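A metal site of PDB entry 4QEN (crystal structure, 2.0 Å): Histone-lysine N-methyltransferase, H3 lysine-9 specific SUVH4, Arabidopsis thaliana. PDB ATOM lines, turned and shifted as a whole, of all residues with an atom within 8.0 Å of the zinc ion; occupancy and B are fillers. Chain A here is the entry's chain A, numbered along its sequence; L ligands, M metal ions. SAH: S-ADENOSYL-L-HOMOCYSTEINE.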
ATOM      1  N   HIS A 461      -4.090  19.102  18.843  1.00  0.00           N
ATOM      2  CA  HIS A 461      -3.545  19.442  17.535  1.00  0.00           C
ATOM      3  C   HIS A 461      -2.252  18.690  17.258  1.00  0.00           C
ATOM      4  O   HIS A 461      -1.426  18.513  18.157  1.00  0.00           O
ATOM      5  CB  HIS A 461      -3.236  20.941  17.474  1.00  0.00           C
ATOM      6  CG  HIS A 461      -2.308  21.308  16.363  1.00  0.00           C
ATOM      7  ND1 HIS A 461      -2.738  21.537  15.079  1.00  0.00           N
ATOM      8  CD2 HIS A 461      -0.956  21.468  16.339  1.00  0.00           C
ATOM      9  CE1 HIS A 461      -1.704  21.819  14.305  1.00  0.00           C
ATOM     10  NE2 HIS A 461      -0.610  21.773  15.052  1.00  0.00           N
ATOM     11  N   SER A 462      -2.052  18.274  16.015  1.00  0.00           N
ATOM     12  CA  SER A 462      -0.733  17.856  15.566  1.00  0.00           C
ATOM     13  C   SER A 462      -0.384  18.452  14.206  1.00  0.00           C
ATOM     14  O   SER A 462      -1.262  18.642  13.368  1.00  0.00           O
ATOM     15  CB  SER A 462      -0.615  16.336  15.504  1.00  0.00           C
ATOM     16  OG  SER A 462       0.647  15.952  14.950  1.00  0.00           O
ATOM     17  N   CYS A 463       0.890  18.741  13.996  1.00  0.00           N
ATOM     18  CA  CYS A 463       1.377  19.156  12.690  1.00  0.00           C
ATOM     19  C   CYS A 463       1.451  17.963  11.712  1.00  0.00           C
ATOM     20  O   CYS A 463       1.535  18.160  10.508  1.00  0.00           O
ATOM     21  CB  CYS A 463       2.736  19.853  12.831  1.00  0.00           C
ATOM     22  SG  CYS A 463       2.715  21.276  14.023  1.00  0.00           S
ATOM     23  N   GLU A 464       1.413  16.745  12.264  1.00  0.00           N
ATOM     24  CA  GLU A 464       1.273  15.525  11.443  1.00  0.00           C
ATOM     25  C   GLU A 464       0.137  14.648  11.966  1.00  0.00           C
ATOM     26  O   GLU A 464       0.340  13.602  12.579  1.00  0.00           O
ATOM     27  CB  GLU A 464       2.593  14.733  11.370  1.00  0.00           C
ATOM     28  CG  GLU A 464       3.112  14.193  12.695  1.00  0.00           C
ATOM     29  CD  GLU A 464       3.671  12.778  12.606  1.00  0.00           C
ATOM     30  OE1 GLU A 464       3.767  12.228  11.488  1.00  0.00           O
ATOM     31  OE2 GLU A 464       4.016  12.223  13.668  1.00  0.00           O
ATOM     32  N   ALA A 520       3.091  27.735  21.760  1.00  0.00           N
ATOM     33  CA  ALA A 520       4.015  26.669  21.361  1.00  0.00           C
ATOM     34  C   ALA A 520       3.299  25.349  21.054  1.00  0.00           C
ATOM     35  O   ALA A 520       2.315  24.985  21.714  1.00  0.00           O
ATOM     36  CB  ALA A 520       5.076  26.466  22.441  1.00  0.00           C
ATOM     37  N   CYS A 521       3.765  24.641  20.036  1.00  0.00           N
ATOM     38  CA  CYS A 521       3.240  23.313  19.736  1.00  0.00           C
ATOM     39  C   CYS A 521       4.118  22.235  20.342  1.00  0.00           C
ATOM     40  O   CYS A 521       5.346  22.276  20.231  1.00  0.00           O
ATOM     41  CB  CYS A 521       3.142  23.080  18.225  1.00  0.00           C
ATOM     42  SG  CYS A 521       2.383  21.494  17.853  1.00  0.00           S
ATOM     43  N   TYR A 522       3.484  21.248  20.965  1.00  0.00           N
ATOM     44  CA  TYR A 522       4.221  20.138  21.559  1.00  0.00           C
ATOM     45  C   TYR A 522       3.848  18.804  20.915  1.00  0.00           C
ATOM     46  O   TYR A 522       3.923  17.774  21.567  1.00  0.00           O
ATOM     47  CB  TYR A 522       3.941  20.079  23.065  1.00  0.00           C
ATOM     48  CG  TYR A 522       4.716  21.079  23.888  1.00  0.00           C
ATOM     49  CD1 TYR A 522       5.962  20.764  24.423  1.00  0.00           C
ATOM     50  CD2 TYR A 522       4.196  22.341  24.132  1.00  0.00           C
ATOM     51  CE1 TYR A 522       6.661  21.688  25.181  1.00  0.00           C
ATOM     52  CE2 TYR A 522       4.894  23.277  24.880  1.00  0.00           C
ATOM     53  CZ  TYR A 522       6.123  22.938  25.402  1.00  0.00           C
ATOM     54  OH  TYR A 522       6.818  23.857  26.153  1.00  0.00           O
ATOM     55  N   CYS A 523       3.430  18.825  19.645  1.00  0.00           N
ATOM     56  CA  CYS A 523       2.916  17.597  19.034  1.00  0.00           C
ATOM     57  C   CYS A 523       3.997  16.542  18.853  1.00  0.00           C
ATOM     58  O   CYS A 523       3.706  15.364  18.654  1.00  0.00           O
ATOM     59  CB  CYS A 523       2.208  17.888  17.694  1.00  0.00           C
ATOM     60  SG  CYS A 523       3.307  18.210  16.279  1.00  0.00           S
ATOM     61  N   GLY A 524       5.262  16.974  18.912  1.00  0.00           N
ATOM     62  CA  GLY A 524       6.389  16.063  18.863  1.00  0.00           C
ATOM     63  C   GLY A 524       6.695  15.521  17.475  1.00  0.00           C
ATOM     64  O   GLY A 524       7.530  14.634  17.309  1.00  0.00           O
ATOM     65  N   ALA A 525       6.026  16.075  16.470  1.00  0.00           N
ATOM     66  CA  ALA A 525       6.185  15.596  15.101  1.00  0.00           C
ATOM     67  C   ALA A 525       7.577  15.913  14.606  1.00  0.00           C
ATOM     68  O   ALA A 525       8.232  16.806  15.134  1.00  0.00           O
ATOM     69  CB  ALA A 525       5.190  16.241  14.201  1.00  0.00           C
ATOM     70  N   LEU A 526       8.010  15.198  13.583  1.00  0.00           N
ATOM     71  CA  LEU A 526       9.313  15.470  12.985  1.00  0.00           C
ATOM     72  C   LEU A 526       9.313  16.851  12.342  1.00  0.00           C
ATOM     73  O   LEU A 526      10.258  17.604  12.505  1.00  0.00           O
ATOM     74  CB  LEU A 526       9.676  14.381  11.959  1.00  0.00           C
ATOM     75  CG  LEU A 526      10.493  13.161  12.406  1.00  0.00           C
ATOM     76  CD1 LEU A 526       9.811  12.380  13.529  1.00  0.00           C
ATOM     77  CD2 LEU A 526      10.776  12.243  11.228  1.00  0.00           C
ATOM     78  N   ASN A 527       8.252  17.200  11.628  1.00  0.00           N
ATOM     79  CA  ASN A 527       8.162  18.510  10.968  1.00  0.00           C
ATOM     80  C   ASN A 527       7.339  19.557  11.734  1.00  0.00           C
ATOM     81  O   ASN A 527       6.594  20.340  11.131  1.00  0.00           O
ATOM     82  CB  ASN A 527       7.603  18.339   9.543  1.00  0.00           C
ATOM     83  CG  ASN A 527       6.122  17.999   9.527  1.00  0.00           C
ATOM     84  OD1 ASN A 527       5.540  17.610  10.546  1.00  0.00           O
ATOM     85  ND2 ASN A 527       5.484  18.146   8.361  1.00  0.00           N
ATOM     86  N   CYS A 528       7.479  19.578  13.053  1.00  0.00           N
ATOM     87  CA  CYS A 528       6.549  20.318  13.935  1.00  0.00           C
ATOM     88  C   CYS A 528       6.288  21.822  13.687  1.00  0.00           C
ATOM     89  O   CYS A 528       5.247  22.303  14.058  1.00  0.00           O
ATOM     90  CB  CYS A 528       6.888  20.083  15.408  1.00  0.00           C
ATOM     91  SG  CYS A 528       5.880  21.071  16.555  1.00  0.00           S
ATOM     92  N   ARG A 529       7.212  22.578  13.113  1.00  0.00           N
ATOM     93  CA  ARG A 529       6.976  24.029  12.932  1.00  0.00           C
ATOM     94  C   ARG A 529       6.821  24.837  14.251  1.00  0.00           C
ATOM     95  O   ARG A 529       6.984  26.055  14.242  1.00  0.00           O
ATOM     96  CB  ARG A 529       5.775  24.322  11.991  1.00  0.00           C
ATOM     97  CG  ARG A 529       4.527  24.853  12.695  1.00  0.00           C
ATOM     98  CD  ARG A 529       3.448  25.342  11.737  1.00  0.00           C
ATOM     99  NE  ARG A 529       2.286  25.860  12.481  1.00  0.00           N
ATOM    100  CZ  ARG A 529       1.256  26.496  11.921  1.00  0.00           C
ATOM    101  NH1 ARG A 529       1.229  26.719  10.618  1.00  0.00           N
ATOM    102  NH2 ARG A 529       0.254  26.919  12.684  1.00  0.00           N
ATOM    103  N   LYS A 530       6.459  24.150  15.333  1.00  0.00           N
ATOM    104  CA  LYS A 530       6.647  24.637  16.715  1.00  0.00           C
ATOM    105  C   LYS A 530       5.620  25.621  17.295  1.00  0.00           C
ATOM    106  O   LYS A 530       5.771  26.060  18.429  1.00  0.00           O
ATOM    107  CB  LYS A 530       8.068  25.206  16.900  1.00  0.00           C
ATOM    108  CG  LYS A 530       9.154  24.150  16.895  1.00  0.00           C
ATOM    109  CD  LYS A 530       9.006  23.218  18.081  1.00  0.00           C
ATOM    110  CE  LYS A 530      10.074  22.149  18.053  1.00  0.00           C
ATOM    111  NZ  LYS A 530      11.416  22.776  17.868  1.00  0.00           N
ATOM    112  N   ARG A 531       4.577  25.941  16.539  1.00  0.00           N
ATOM    113  CA  ARG A 531       3.557  26.876  17.013  1.00  0.00           C
ATOM    114  C   ARG A 531       2.161  26.444  16.577  1.00  0.00           C
ATOM    115  O   ARG A 531       1.960  26.102  15.407  1.00  0.00           O
ATOM    116  CB  ARG A 531       3.825  28.286  16.493  1.00  0.00           C
ATOM    117  CG  ARG A 531       5.137  28.917  16.932  1.00  0.00           C
ATOM    118  CD  ARG A 531       5.446  30.164  16.116  1.00  0.00           C
ATOM    119  NE  ARG A 531       4.350  31.142  16.142  1.00  0.00           N
ATOM    120  CZ  ARG A 531       4.391  32.338  15.565  1.00  0.00           C
ATOM    121  NH1 ARG A 531       5.473  32.713  14.899  1.00  0.00           N
ATOM    122  NH2 ARG A 531       3.355  33.161  15.648  1.00  0.00           N
ATOM    123  N   LEU A 532       1.194  26.454  17.496  1.00  0.00           N
ATOM    124  CA  LEU A 532      -0.193  26.260  17.109  1.00  0.00           C
ATOM    125  C   LEU A 532      -0.579  27.509  16.355  1.00  0.00           C
ATOM    126  O   LEU A 532      -1.307  27.462  15.350  1.00  0.00           O
ATOM    127  CB  LEU A 532      -1.104  26.056  18.323  1.00  0.00           C
ATOM    128  CG  LEU A 532      -1.539  24.625  18.625  1.00  0.00           C
ATOM    129  CD1 LEU A 532      -0.330  23.793  19.052  1.00  0.00           C
ATOM    130  CD2 LEU A 532      -2.620  24.590  19.693  1.00  0.00           C
HETATM  131  N   SAH L   1      -5.578  19.510  25.655  1.00  0.00           N
HETATM  132  CA  SAH L   1      -6.868  20.140  25.883  1.00  0.00           C
HETATM  133  CB  SAH L   1      -7.904  19.624  24.886  1.00  0.00           C
HETATM  134  CG  SAH L   1      -7.757  20.236  23.501  1.00  0.00           C
HETATM  135  SD  SAH L   1      -8.500  21.886  23.494  1.00  0.00           S
HETATM  136  C   SAH L   1      -7.375  19.963  27.313  1.00  0.00           C
HETATM  137  O   SAH L   1      -8.558  20.167  27.581  1.00  0.00           O
HETATM  138  OXT SAH L   1      -6.620  19.609  28.213  1.00  0.00           O
HETATM  139  C5' SAH L   1      -7.089  22.689  22.699  1.00  0.00           C
HETATM  140  C4' SAH L   1      -6.065  23.236  23.688  1.00  0.00           C
HETATM  141  O4' SAH L   1      -5.203  22.189  24.109  1.00  0.00           O
HETATM  142  C3' SAH L   1      -5.203  24.307  23.054  1.00  0.00           C
HETATM  143  O3' SAH L   1      -5.664  25.602  23.339  1.00  0.00           O
HETATM  144  C2' SAH L   1      -3.855  24.082  23.700  1.00  0.00           C
HETATM  145  O2' SAH L   1      -3.796  24.750  24.933  1.00  0.00           O
HETATM  146  C1' SAH L   1      -3.852  22.593  23.985  1.00  0.00           C
HETATM  147  N9  SAH L   1      -3.195  21.895  22.868  1.00  0.00           N
HETATM  148  C8  SAH L   1      -3.801  21.131  21.891  1.00  0.00           C
HETATM  149  N7  SAH L   1      -2.833  20.671  21.048  1.00  0.00           N
HETATM  150  C5  SAH L   1      -1.633  21.134  21.471  1.00  0.00           C
HETATM  151  C6  SAH L   1      -0.331  20.968  20.982  1.00  0.00           C
HETATM  152  N6  SAH L   1      -0.089  20.239  19.898  1.00  0.00           N
HETATM  153  N1  SAH L   1       0.712  21.588  21.652  1.00  0.00           N
HETATM  154  C2  SAH L   1       0.482  22.346  22.777  1.00  0.00           C
HETATM  155  N3  SAH L   1      -0.810  22.502  23.254  1.00  0.00           N
HETATM  156  C4  SAH L   1      -1.845  21.904  22.618  1.00  0.00           C
HETATM  157 ZN    ZN M   1       3.616  20.542  16.162  1.00  0.00          ZN
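Four residues have an atom within 4 Å of the zinc ion: Cys 463, Cys 521, Cys 523 and Cys 528.
A nitrogen (N6) of the ligand lies close to the side-chain sulfur (SG) of Cys 521 (3.4 Å).
The backbone NH (N) of His 461 is in hydrogen-bond range of a nitrogen (N7) of the ligand.
The backbone carbonyl oxygen (O) of His 461 lies within hydrogen-bond range of a nitrogen (N6) of the ligand (2.8 Å).
N of Tyr 522 is in hydrogen-bond range of N1 of the ligand, 2.9 Å away.
The backbone carbonyl oxygen (O) of Lys 530 is in hydrogen-bond range of the backbone NH (N) of Cys 521, at 2.9 Å.
The side-chain hydroxyl (OG) of Ser 462 sits close to the side-chain sulfur (SG) of Cys 523 (3.7 Å).
SG of Cys 523 lies close to N of Ala 525 (3.5 Å).
The backbone NH (N) of Lys 530 lies close to the side-chain sulfur (SG) of Cys 528 (3.4 Å).
SG of Cys 463 sits close to NE2 of His 461, at 3.5 Å.
SG of Cys 521 binds the zinc ion, 2.3 Å away.
SG of Cys 523 is bound to the zinc ion (2.4 Å).
The side-chain sulfur (SG) of Cys 528 binds the zinc ion (2.4 Å).
The zinc ion is bound by the side-chain sulfur (SG) of Cys 463, 2.4 Å away.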
